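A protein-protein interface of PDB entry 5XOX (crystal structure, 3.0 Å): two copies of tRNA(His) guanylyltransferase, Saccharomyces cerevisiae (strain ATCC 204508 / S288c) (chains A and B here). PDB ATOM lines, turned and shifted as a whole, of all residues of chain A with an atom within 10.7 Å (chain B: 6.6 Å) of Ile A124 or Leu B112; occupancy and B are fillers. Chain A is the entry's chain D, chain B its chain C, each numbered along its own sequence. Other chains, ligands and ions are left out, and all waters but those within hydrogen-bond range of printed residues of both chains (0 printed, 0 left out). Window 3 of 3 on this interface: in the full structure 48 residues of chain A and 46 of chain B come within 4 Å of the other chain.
O of Pro A128 lies within hydrogen-bond range of OG of Ser B107 (2.9 Å).
ND2 of Asn B60 lies within hydrogen-bond range of OD1 of Asn B108 (3.1 Å).
The backbone carbonyl oxygen (O) of Phe B104 is in hydrogen-bond range of the side-chain amide nitrogen (ND2) of Asn B108.
Among the printed residues, pairs that only touch across the chains: Ser A107 with Val B110 (3.5 Å), Val A110 with Ser B107 (3.4 Å), Val A110 with Val B110 (3.5 Å), Val A110 with Ala B111 (3.6 Å), Ala A111 with Val B110 (3.7 Å), Ile A124 with Leu B112 (3.995 Å), Leu A127 with Ser B107 (3.4 Å), Leu A127 with Asn B108 (3.1 Å) and Tyr A129 with Phe B104 (3.8 Å).
Phe A39 touches none of the printed residues of chain B.
Of the printed residues of chain B, Ser A107 touches Val B110.
Printed residues of chain B within 4 Å of Val A110: Ser B107 (3.4 Å), Val B110 (3.5 Å) and Ala B111 (3.6 Å).
Of the printed residues of chain B, Ala A111 touches Val B110 (3.7 Å).
Leu A122 touches none of the printed residues of chain B.
Of the printed residues of chain B, Ile A124 touches Leu B112 (3.995 Å).
Of the printed residues of chain A, Phe B104 touches Tyr A129.
Asn B108 touches just one residue of chain A: Leu A127.
Of the printed residues of chain A, Val B110 touches Ser A107, Val A110 and Ala A111.
Of the printed residues of chain A, Ala B111 touches Val A110.
Printed residues of chain A within 4 Å of Leu B112: Ile A124 (3.995 Å).
No residue of chain A comes within 4 Å of Ala B114.
No residue of chain A comes within 4 Å of Phe B116.
The nearest printed residue of chain A that does not touch Leu B112 is Val A110 (6.4 Å).
The nearest printed residue of chain B that does not touch Leu A127 is Ala B111 (4.5 Å).
Of the 16 printed residues of chain B, 6 touch a printed residue of chain A.
Printed residues of chain B that touch a printed residue of chain A: Phe B104, Ser B107, Asn B108, Val B110, Ala B111 and Leu B112.
Of the 17 printed residues of chain A, 7 touch a printed residue of chain B.
Hydrophobic or aromatic side chains of chain A that line the printed part of chain B: Val A110, Ile A124, Leu A127, Pro A128 and Tyr A129.
Ser A107 touches Val B110, and with the chains exchanged Val A110 touches Ser B107.
Val A110 touches its own counterpart, Val B110.
Val A110 touches Ala B111, and with the chains exchanged Ala A111 touches Val B110.
4 positions are printed for both chains.
Of the 10 pairs that touch across the chains among the printed residues, 5 have their exchanged pair printed and touching as well.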
ATOM      1  N   PHE A  36       9.037   4.876 -30.150  1.00  0.00           N
ATOM      2  CA  PHE A  36       8.008   4.339 -29.303  1.00  0.00           C
ATOM      3  C   PHE A  36       8.414   3.019 -28.668  1.00  0.00           C
ATOM      4  O   PHE A  36       8.136   2.762 -27.501  1.00  0.00           O
ATOM      5  CB  PHE A  36       6.772   4.109 -30.097  1.00  0.00           C
ATOM      6  CG  PHE A  36       5.646   3.654 -29.276  1.00  0.00           C
ATOM      7  CD1 PHE A  36       5.110   4.492 -28.318  1.00  0.00           C
ATOM      8  CD2 PHE A  36       5.170   2.365 -29.393  1.00  0.00           C
ATOM      9  CE1 PHE A  36       4.060   4.085 -27.550  1.00  0.00           C
ATOM     10  CE2 PHE A  36       4.128   1.943 -28.614  1.00  0.00           C
ATOM     11  CZ  PHE A  36       3.571   2.808 -27.687  1.00  0.00           C
ATOM     12  N   PHE A  39      11.107   3.930 -25.939  1.00  0.00           N
ATOM     13  CA  PHE A  39      10.645   4.489 -24.673  1.00  0.00           C
ATOM     14  C   PHE A  39      10.140   3.401 -23.732  1.00  0.00           C
ATOM     15  O   PHE A  39      10.448   3.417 -22.536  1.00  0.00           O
ATOM     16  CB  PHE A  39       9.545   5.528 -24.926  1.00  0.00           C
ATOM     17  CG  PHE A  39       9.084   6.267 -23.691  1.00  0.00           C
ATOM     18  CD1 PHE A  39       8.123   5.724 -22.844  1.00  0.00           C
ATOM     19  CD2 PHE A  39       9.602   7.516 -23.392  1.00  0.00           C
ATOM     20  CE1 PHE A  39       7.693   6.409 -21.712  1.00  0.00           C
ATOM     21  CE2 PHE A  39       9.183   8.208 -22.265  1.00  0.00           C
ATOM     22  CZ  PHE A  39       8.222   7.655 -21.422  1.00  0.00           C
ATOM     23  N   TYR A  40       9.380   2.446 -24.255  1.00  0.00           N
ATOM     24  CA  TYR A  40       8.772   1.474 -23.365  1.00  0.00           C
ATOM     25  C   TYR A  40       9.693   0.289 -23.230  1.00  0.00           C
ATOM     26  O   TYR A  40       9.392  -0.699 -22.544  1.00  0.00           O
ATOM     27  CB  TYR A  40       7.400   1.079 -23.858  1.00  0.00           C
ATOM     28  CG  TYR A  40       6.465   2.259 -23.736  1.00  0.00           C
ATOM     29  CD1 TYR A  40       6.449   3.264 -24.696  1.00  0.00           C
ATOM     30  CD2 TYR A  40       5.584   2.365 -22.674  1.00  0.00           C
ATOM     31  CE1 TYR A  40       5.590   4.356 -24.586  1.00  0.00           C
ATOM     32  CE2 TYR A  40       4.728   3.456 -22.555  1.00  0.00           C
ATOM     33  CZ  TYR A  40       4.733   4.443 -23.512  1.00  0.00           C
ATOM     34  OH  TYR A  40       3.878   5.516 -23.389  1.00  0.00           O
ATOM     35  N   SER A 107      -7.602   2.127 -31.273  1.00  0.00           N
ATOM     36  CA  SER A 107      -8.465   2.073 -30.101  1.00  0.00           C
ATOM     37  C   SER A 107      -8.288   0.734 -29.418  1.00  0.00           C
ATOM     38  O   SER A 107      -8.222   0.654 -28.189  1.00  0.00           O
ATOM     39  CB  SER A 107      -9.931   2.301 -30.501  1.00  0.00           C
ATOM     40  OG  SER A 107     -10.809   2.344 -29.385  1.00  0.00           O
ATOM     41  N   VAL A 110      -4.519   0.762 -27.687  1.00  0.00           N
ATOM     42  CA  VAL A 110      -4.594   1.399 -26.361  1.00  0.00           C
ATOM     43  C   VAL A 110      -5.375   0.543 -25.372  1.00  0.00           C
ATOM     44  O   VAL A 110      -4.853   0.225 -24.302  1.00  0.00           O
ATOM     45  CB  VAL A 110      -5.202   2.835 -26.436  1.00  0.00           C
ATOM     46  CG1 VAL A 110      -5.202   3.482 -25.075  1.00  0.00           C
ATOM     47  CG2 VAL A 110      -4.386   3.722 -27.384  1.00  0.00           C
ATOM     48  N   ALA A 111      -6.587   0.130 -25.744  1.00  0.00           N
ATOM     49  CA  ALA A 111      -7.429  -0.708 -24.871  1.00  0.00           C
ATOM     50  C   ALA A 111      -6.723  -1.955 -24.335  1.00  0.00           C
ATOM     51  O   ALA A 111      -6.723  -2.225 -23.120  1.00  0.00           O
ATOM     52  CB  ALA A 111      -8.691  -1.129 -25.609  1.00  0.00           C
ATOM     53  N   TRP A 113      -3.571  -2.676 -24.243  1.00  0.00           N
ATOM     54  CA  TRP A 113      -2.232  -2.529 -23.688  1.00  0.00           C
ATOM     55  C   TRP A 113      -2.105  -3.164 -22.315  1.00  0.00           C
ATOM     56  O   TRP A 113      -1.182  -3.950 -22.083  1.00  0.00           O
ATOM     57  CB  TRP A 113      -1.820  -1.068 -23.608  1.00  0.00           C
ATOM     58  CG  TRP A 113      -0.396  -0.868 -23.092  1.00  0.00           C
ATOM     59  CD1 TRP A 113       0.016  -0.823 -21.783  1.00  0.00           C
ATOM     60  CD2 TRP A 113       0.801  -0.743 -23.886  1.00  0.00           C
ATOM     61  NE1 TRP A 113       1.382  -0.627 -21.723  1.00  0.00           N
ATOM     62  CE2 TRP A 113       1.882  -0.582 -22.998  1.00  0.00           C
ATOM     63  CE3 TRP A 113       1.055  -0.732 -25.261  1.00  0.00           C
ATOM     64  CZ2 TRP A 113       3.186  -0.417 -23.443  1.00  0.00           C
ATOM     65  CZ3 TRP A 113       2.343  -0.567 -25.695  1.00  0.00           C
ATOM     66  CH2 TRP A 113       3.394  -0.412 -24.792  1.00  0.00           C
ATOM     67  N   LYS A 120       5.097  -1.956 -17.835  1.00  0.00           N
ATOM     68  CA  LYS A 120       5.197  -0.502 -17.971  1.00  0.00           C
ATOM     69  C   LYS A 120       3.919   0.056 -18.618  1.00  0.00           C
ATOM     70  O   LYS A 120       3.637  -0.254 -19.765  1.00  0.00           O
ATOM     71  CB  LYS A 120       6.446  -0.138 -18.796  1.00  0.00           C
ATOM     72  CG  LYS A 120       6.680   1.368 -19.056  1.00  0.00           C
ATOM     73  CD  LYS A 120       7.288   2.072 -17.826  1.00  0.00           C
ATOM     74  CE  LYS A 120       7.587   3.550 -18.080  1.00  0.00           C
ATOM     75  NZ  LYS A 120       8.766   3.738 -18.978  1.00  0.00           N
ATOM     76  N   PRO A 121       3.121   0.842 -17.873  1.00  0.00           N
ATOM     77  CA  PRO A 121       1.916   1.528 -18.378  1.00  0.00           C
ATOM     78  C   PRO A 121       2.245   2.660 -19.344  1.00  0.00           C
ATOM     79  O   PRO A 121       3.435   2.913 -19.538  1.00  0.00           O
ATOM     80  CB  PRO A 121       1.278   2.095 -17.114  1.00  0.00           C
ATOM     81  CG  PRO A 121       1.717   1.166 -16.047  1.00  0.00           C
ATOM     82  CD  PRO A 121       3.145   0.820 -16.405  1.00  0.00           C
ATOM     83  N   LEU A 122       1.236   3.361 -19.869  1.00  0.00           N
ATOM     84  CA  LEU A 122       1.409   4.251 -21.033  1.00  0.00           C
ATOM     85  C   LEU A 122       2.037   5.651 -20.862  1.00  0.00           C
ATOM     86  O   LEU A 122       2.408   6.295 -21.851  1.00  0.00           O
ATOM     87  CB  LEU A 122       0.037   4.433 -21.695  1.00  0.00           C
ATOM     88  CG  LEU A 122      -0.360   3.634 -22.939  1.00  0.00           C
ATOM     89  CD1 LEU A 122       0.221   4.267 -24.186  1.00  0.00           C
ATOM     90  CD2 LEU A 122       0.215   2.273 -22.802  1.00  0.00           C
ATOM     91  N   ASN A 123       2.157   6.121 -19.626  1.00  0.00           N
ATOM     92  CA  ASN A 123       2.516   7.511 -19.352  1.00  0.00           C
ATOM     93  C   ASN A 123       1.518   8.345 -20.154  1.00  0.00           C
ATOM     94  O   ASN A 123       0.368   7.942 -20.300  1.00  0.00           O
ATOM     95  CB  ASN A 123       3.975   7.813 -19.756  1.00  0.00           C
ATOM     96  CG  ASN A 123       4.544   9.056 -19.075  1.00  0.00           C
ATOM     97  OD1 ASN A 123       4.408  10.171 -19.575  1.00  0.00           O
ATOM     98  ND2 ASN A 123       5.238   8.854 -17.955  1.00  0.00           N
ATOM     99  N   ILE A 124       1.938   9.479 -20.699  1.00  0.00           N
ATOM    100  CA  ILE A 124       1.069  10.270 -21.584  1.00  0.00           C
ATOM    101  C   ILE A 124       1.853  10.786 -22.760  1.00  0.00           C
ATOM    102  O   ILE A 124       1.495  10.568 -23.904  1.00  0.00           O
ATOM    103  CB  ILE A 124       0.367  11.431 -20.862  1.00  0.00           C
ATOM    104  CG1 ILE A 124      -0.951  10.951 -20.280  1.00  0.00           C
ATOM    105  CG2 ILE A 124       0.028  12.543 -21.843  1.00  0.00           C
ATOM    106  CD1 ILE A 124      -1.966  10.660 -21.343  1.00  0.00           C
ATOM    107  N   LYS A 125       2.900  11.538 -22.432  1.00  0.00           N
ATOM    108  CA  LYS A 125       3.674  12.329 -23.375  1.00  0.00           C
ATOM    109  C   LYS A 125       4.051  11.468 -24.581  1.00  0.00           C
ATOM    110  O   LYS A 125       4.164  11.967 -25.701  1.00  0.00           O
ATOM    111  CB  LYS A 125       4.930  12.909 -22.675  1.00  0.00           C
ATOM    112  CG  LYS A 125       4.790  13.172 -21.133  1.00  0.00           C
ATOM    113  CD  LYS A 125       6.159  13.229 -20.378  1.00  0.00           C
ATOM    114  CE  LYS A 125       5.977  13.317 -18.852  1.00  0.00           C
ATOM    115  NZ  LYS A 125       7.240  13.168 -18.086  1.00  0.00           N
ATOM    116  N   HIS A 126       4.178  10.162 -24.351  1.00  0.00           N
ATOM    117  CA  HIS A 126       4.503   9.221 -25.417  1.00  0.00           C
ATOM    118  C   HIS A 126       3.393   8.175 -25.672  1.00  0.00           C
ATOM    119  O   HIS A 126       3.160   7.275 -24.862  1.00  0.00           O
ATOM    120  CB  HIS A 126       5.837   8.537 -25.098  1.00  0.00           C
ATOM    121  CG  HIS A 126       6.916   9.491 -24.680  1.00  0.00           C
ATOM    122  ND1 HIS A 126       6.869  10.202 -23.501  1.00  0.00           N
ATOM    123  CD2 HIS A 126       8.054   9.880 -25.305  1.00  0.00           C
ATOM    124  CE1 HIS A 126       7.938  10.972 -23.405  1.00  0.00           C
ATOM    125  NE2 HIS A 126       8.675  10.795 -24.488  1.00  0.00           N
ATOM    126  N   LEU A 127       2.742   8.300 -26.829  1.00  0.00           N
ATOM    127  CA  LEU A 127       1.574   7.491 -27.188  1.00  0.00           C
ATOM    128  C   LEU A 127       1.704   6.801 -28.529  1.00  0.00           C
ATOM    129  O   LEU A 127       2.456   7.256 -29.395  1.00  0.00           O
ATOM    130  CB  LEU A 127       0.313   8.370 -27.189  1.00  0.00           C
ATOM    131  CG  LEU A 127      -0.700   8.085 -26.066  1.00  0.00           C
ATOM    132  CD1 LEU A 127      -0.063   7.968 -24.688  1.00  0.00           C
ATOM    133  CD2 LEU A 127      -1.942   9.008 -26.084  1.00  0.00           C
ATOM    134  N   PRO A 128       0.987   5.679 -28.704  1.00  0.00           N
ATOM    135  CA  PRO A 128       0.882   5.057 -30.016  1.00  0.00           C
ATOM    136  C   PRO A 128      -0.075   5.858 -30.869  1.00  0.00           C
ATOM    137  O   PRO A 128      -1.084   6.323 -30.334  1.00  0.00           O
ATOM    138  CB  PRO A 128       0.302   3.684 -29.706  1.00  0.00           C
ATOM    139  CG  PRO A 128      -0.503   3.896 -28.516  1.00  0.00           C
ATOM    140  CD  PRO A 128       0.193   4.957 -27.703  1.00  0.00           C
ATOM    141  N   TYR A 129       0.244   6.053 -32.143  1.00  0.00           N
ATOM    142  CA  TYR A 129      -0.737   6.521 -33.112  1.00  0.00           C
ATOM    143  C   TYR A 129      -0.313   6.062 -34.501  1.00  0.00           C
ATOM    144  O   TYR A 129       0.890   5.904 -34.731  1.00  0.00           O
ATOM    145  CB  TYR A 129      -0.938   8.032 -32.988  1.00  0.00           C
ATOM    146  CG  TYR A 129       0.256   8.937 -33.178  1.00  0.00           C
ATOM    147  CD1 TYR A 129       1.301   8.941 -32.279  1.00  0.00           C
ATOM    148  CD2 TYR A 129       0.308   9.830 -34.236  1.00  0.00           C
ATOM    149  CE1 TYR A 129       2.385   9.808 -32.440  1.00  0.00           C
ATOM    150  CE2 TYR A 129       1.378  10.689 -34.413  1.00  0.00           C
ATOM    151  CZ  TYR A 129       2.417  10.682 -33.517  1.00  0.00           C
ATOM    152  OH  TYR A 129       3.486  11.547 -33.698  1.00  0.00           O
ATOM    153  N   LEU B  53     -13.690  15.204 -21.795  1.00  0.00           N
ATOM    154  CA  LEU B  53     -12.692  14.252 -22.244  1.00  0.00           C
ATOM    155  C   LEU B  53     -12.300  14.586 -23.691  1.00  0.00           C
ATOM    156  O   LEU B  53     -11.111  14.722 -24.048  1.00  0.00           O
ATOM    157  CB  LEU B  53     -13.254  12.833 -22.133  1.00  0.00           C
ATOM    158  CG  LEU B  53     -12.689  11.734 -23.030  1.00  0.00           C
ATOM    159  CD1 LEU B  53     -11.201  11.562 -22.743  1.00  0.00           C
ATOM    160  CD2 LEU B  53     -13.426  10.428 -22.763  1.00  0.00           C
ATOM    161  N   ALA B  56     -10.098  17.211 -23.802  1.00  0.00           N
ATOM    162  CA  ALA B  56      -8.738  16.887 -23.370  1.00  0.00           C
ATOM    163  C   ALA B  56      -7.914  16.411 -24.561  1.00  0.00           C
ATOM    164  O   ALA B  56      -6.791  16.893 -24.794  1.00  0.00           O
ATOM    165  CB  ALA B  56      -8.745  15.829 -22.262  1.00  0.00           C
ATOM    166  N   CYS B  57      -8.487  15.472 -25.312  1.00  0.00           N
ATOM    167  CA  CYS B  57      -7.821  14.951 -26.497  1.00  0.00           C
ATOM    168  C   CYS B  57      -7.463  16.125 -27.416  1.00  0.00           C
ATOM    169  O   CYS B  57      -6.321  16.265 -27.857  1.00  0.00           O
ATOM    170  CB  CYS B  57      -8.724  13.973 -27.216  1.00  0.00           C
ATOM    171  SG  CYS B  57      -9.304  12.704 -26.150  1.00  0.00           S
ATOM    172  N   ASN B  60      -4.593  18.195 -26.289  1.00  0.00           N
ATOM    173  CA  ASN B  60      -3.327  17.473 -26.453  1.00  0.00           C
ATOM    174  C   ASN B  60      -2.906  17.415 -27.925  1.00  0.00           C
ATOM    175  O   ASN B  60      -1.713  17.315 -28.224  1.00  0.00           O
ATOM    176  CB  ASN B  60      -3.414  16.047 -25.899  1.00  0.00           C
ATOM    177  CG  ASN B  60      -3.672  16.014 -24.405  1.00  0.00           C
ATOM    178  OD1 ASN B  60      -3.653  17.045 -23.728  1.00  0.00           O
ATOM    179  ND2 ASN B  60      -3.913  14.824 -23.881  1.00  0.00           N
ATOM    180  N   PHE B 104      -4.393   9.619 -33.411  1.00  0.00           N
ATOM    181  CA  PHE B 104      -3.894  10.313 -32.242  1.00  0.00           C
ATOM    182  C   PHE B 104      -5.034  10.617 -31.279  1.00  0.00           C
ATOM    183  O   PHE B 104      -4.995  10.250 -30.106  1.00  0.00           O
ATOM    184  CB  PHE B 104      -3.237  11.614 -32.638  1.00  0.00           C
ATOM    185  CG  PHE B 104      -2.558  12.300 -31.503  1.00  0.00           C
ATOM    186  CD1 PHE B 104      -1.610  11.608 -30.758  1.00  0.00           C
ATOM    187  CD2 PHE B 104      -2.871  13.600 -31.145  1.00  0.00           C
ATOM    188  CE1 PHE B 104      -0.958  12.195 -29.720  1.00  0.00           C
ATOM    189  CE2 PHE B 104      -2.216  14.199 -30.087  1.00  0.00           C
ATOM    190  CZ  PHE B 104      -1.257  13.488 -29.376  1.00  0.00           C
ATOM    191  N   SER B 107      -6.480   7.517 -29.742  1.00  0.00           N
ATOM    192  CA  SER B 107      -5.519   7.053 -28.742  1.00  0.00           C
ATOM    193  C   SER B 107      -5.681   7.822 -27.432  1.00  0.00           C
ATOM    194  O   SER B 107      -5.841   7.222 -26.363  1.00  0.00           O
ATOM    195  CB  SER B 107      -4.080   7.193 -29.270  1.00  0.00           C
ATOM    196  OG  SER B 107      -3.118   6.705 -28.342  1.00  0.00           O
ATOM    197  N   ASN B 108      -5.674   9.147 -27.536  1.00  0.00           N
ATOM    198  CA  ASN B 108      -5.970  10.044 -26.415  1.00  0.00           C
ATOM    199  C   ASN B 108      -7.290   9.798 -25.679  1.00  0.00           C
ATOM    200  O   ASN B 108      -7.359   9.887 -24.446  1.00  0.00           O
ATOM    201  CB  ASN B 108      -5.937  11.477 -26.920  1.00  0.00           C
ATOM    202  CG  ASN B 108      -4.548  12.016 -26.945  1.00  0.00           C
ATOM    203  OD1 ASN B 108      -4.275  13.076 -26.391  1.00  0.00           O
ATOM    204  ND2 ASN B 108      -3.626  11.231 -27.493  1.00  0.00           N
ATOM    205  N   TYR B 109      -8.334   9.505 -26.434  1.00  0.00           N
ATOM    206  CA  TYR B 109      -9.613   9.204 -25.839  1.00  0.00           C
ATOM    207  C   TYR B 109      -9.511   7.955 -24.986  1.00  0.00           C
ATOM    208  O   TYR B 109      -9.881   7.971 -23.813  1.00  0.00           O
ATOM    209  CB  TYR B 109     -10.626   9.019 -26.912  1.00  0.00           C
ATOM    210  CG  TYR B 109     -12.046   9.135 -26.513  1.00  0.00           C
ATOM    211  CD1 TYR B 109     -12.668  10.363 -26.467  1.00  0.00           C
ATOM    212  CD2 TYR B 109     -12.809   7.995 -26.268  1.00  0.00           C
ATOM    213  CE1 TYR B 109     -14.033  10.460 -26.173  1.00  0.00           C
ATOM    214  CE2 TYR B 109     -14.174   8.078 -25.961  1.00  0.00           C
ATOM    215  CZ  TYR B 109     -14.776   9.309 -25.917  1.00  0.00           C
ATOM    216  OH  TYR B 109     -16.113   9.380 -25.619  1.00  0.00           O
ATOM    217  N   VAL B 110      -8.990   6.875 -25.555  1.00  0.00           N
ATOM    218  CA  VAL B 110      -8.965   5.619 -24.806  1.00  0.00           C
ATOM    219  C   VAL B 110      -8.034   5.698 -23.589  1.00  0.00           C
ATOM    220  O   VAL B 110      -8.369   5.192 -22.505  1.00  0.00           O
ATOM    221  CB  VAL B 110      -8.618   4.454 -25.737  1.00  0.00           C
ATOM    222  CG1 VAL B 110      -8.711   3.127 -25.005  1.00  0.00           C
ATOM    223  CG2 VAL B 110      -9.613   4.444 -26.897  1.00  0.00           C
ATOM    224  N   ALA B 111      -6.902   6.372 -23.748  1.00  0.00           N
ATOM    225  CA  ALA B 111      -6.045   6.657 -22.602  1.00  0.00           C
ATOM    226  C   ALA B 111      -6.814   7.362 -21.494  1.00  0.00           C
ATOM    227  O   ALA B 111      -6.933   6.843 -20.381  1.00  0.00           O
ATOM    228  CB  ALA B 111      -4.873   7.512 -23.019  1.00  0.00           C
ATOM    229  N   LEU B 112      -7.371   8.527 -21.814  1.00  0.00           N
ATOM    230  CA  LEU B 112      -7.960   9.384 -20.789  1.00  0.00           C
ATOM    231  C   LEU B 112      -9.343   8.932 -20.297  1.00  0.00           C
ATOM    232  O   LEU B 112      -9.904   9.518 -19.358  1.00  0.00           O
ATOM    233  CB  LEU B 112      -8.068  10.819 -21.303  1.00  0.00           C
ATOM    234  CG  LEU B 112      -6.790  11.435 -21.866  1.00  0.00           C
ATOM    235  CD1 LEU B 112      -7.129  12.645 -22.754  1.00  0.00           C
ATOM    236  CD2 LEU B 112      -5.768  11.755 -20.790  1.00  0.00           C
ATOM    237  N   TRP B 113      -9.909   7.912 -20.929  1.00  0.00           N
ATOM    238  CA  TRP B 113     -11.158   7.360 -20.429  1.00  0.00           C
ATOM    239  C   TRP B 113     -11.023   6.939 -18.976  1.00  0.00           C
ATOM    240  O   TRP B 113     -11.940   7.151 -18.175  1.00  0.00           O
ATOM    241  CB  TRP B 113     -11.623   6.168 -21.258  1.00  0.00           C
ATOM    242  CG  TRP B 113     -12.966   5.694 -20.825  1.00  0.00           C
ATOM    243  CD1 TRP B 113     -13.275   5.014 -19.670  1.00  0.00           C
ATOM    244  CD2 TRP B 113     -14.208   5.909 -21.504  1.00  0.00           C
ATOM    245  NE1 TRP B 113     -14.627   4.754 -19.622  1.00  0.00           N
ATOM    246  CE2 TRP B 113     -15.222   5.305 -20.728  1.00  0.00           C
ATOM    247  CE3 TRP B 113     -14.560   6.550 -22.694  1.00  0.00           C
ATOM    248  CZ2 TRP B 113     -16.563   5.321 -21.114  1.00  0.00           C
ATOM    249  CZ3 TRP B 113     -15.884   6.560 -23.072  1.00  0.00           C
ATOM    250  CH2 TRP B 113     -16.873   5.949 -22.285  1.00  0.00           C
ATOM    251  N   ALA B 114      -9.887   6.329 -18.649  1.00  0.00           N
ATOM    252  CA  ALA B 114      -9.640   5.871 -17.293  1.00  0.00           C
ATOM    253  C   ALA B 114      -9.877   7.036 -16.319  1.00  0.00           C
ATOM    254  O   ALA B 114     -10.534   6.879 -15.286  1.00  0.00           O
ATOM    255  CB  ALA B 114      -8.222   5.311 -17.174  1.00  0.00           C
ATOM    256  N   LYS B 115      -9.377   8.212 -16.698  1.00  0.00           N
ATOM    257  CA  LYS B 115      -9.531   9.458 -15.930  1.00  0.00           C
ATOM    258  C   LYS B 115     -10.966   9.966 -15.825  1.00  0.00           C
ATOM    259  O   LYS B 115     -11.440  10.249 -14.728  1.00  0.00           O
ATOM    260  CB  LYS B 115      -8.664  10.571 -16.545  1.00  0.00           C
ATOM    261  CG  LYS B 115      -8.645  11.907 -15.779  1.00  0.00           C
ATOM    262  CD  LYS B 115      -7.316  12.660 -15.981  1.00  0.00           C
ATOM    263  CE  LYS B 115      -6.134  11.885 -15.375  1.00  0.00           C
ATOM    264  NZ  LYS B 115      -4.790  12.510 -15.593  1.00  0.00           N
ATOM    265  N   PHE B 116     -11.644  10.120 -16.959  1.00  0.00           N
ATOM    266  CA  PHE B 116     -12.978  10.744 -16.946  1.00  0.00           C
ATOM    267  C   PHE B 116     -14.156   9.831 -16.555  1.00  0.00           C
ATOM    268  O   PHE B 116     -15.198  10.320 -16.108  1.00  0.00           O
ATOM    269  CB  PHE B 116     -13.244  11.390 -18.313  1.00  0.00           C
ATOM    270  CG  PHE B 116     -12.451  12.655 -18.551  1.00  0.00           C
ATOM    271  CD1 PHE B 116     -12.935  13.883 -18.115  1.00  0.00           C
ATOM    272  CD2 PHE B 116     -11.204  12.614 -19.152  1.00  0.00           C
ATOM    273  CE1 PHE B 116     -12.212  15.050 -18.320  1.00  0.00           C
ATOM    274  CE2 PHE B 116     -10.472  13.780 -19.351  1.00  0.00           C
ATOM    275  CZ  PHE B 116     -10.981  14.997 -18.934  1.00  0.00           C
ATOM    276  N   PHE B 117     -13.989   8.520 -16.700  1.00  0.00           N
ATOM    277  CA  PHE B 117     -15.047   7.579 -16.334  1.00  0.00           C
ATOM    278  C   PHE B 117     -14.533   6.410 -15.506  1.00  0.00           C
ATOM    279  O   PHE B 117     -14.331   5.320 -16.037  1.00  0.00           O
ATOM    280  CB  PHE B 117     -15.746   7.002 -17.575  1.00  0.00           C
ATOM    281  CG  PHE B 117     -16.448   8.016 -18.431  1.00  0.00           C
ATOM    282  CD1 PHE B 117     -15.745   8.760 -19.367  1.00  0.00           C
ATOM    283  CD2 PHE B 117     -17.818   8.206 -18.319  1.00  0.00           C
ATOM    284  CE1 PHE B 117     -16.391   9.687 -20.167  1.00  0.00           C
ATOM    285  CE2 PHE B 117     -18.476   9.132 -19.121  1.00  0.00           C
ATOM    286  CZ  PHE B 117     -17.762   9.874 -20.045  1.00  0.00           C
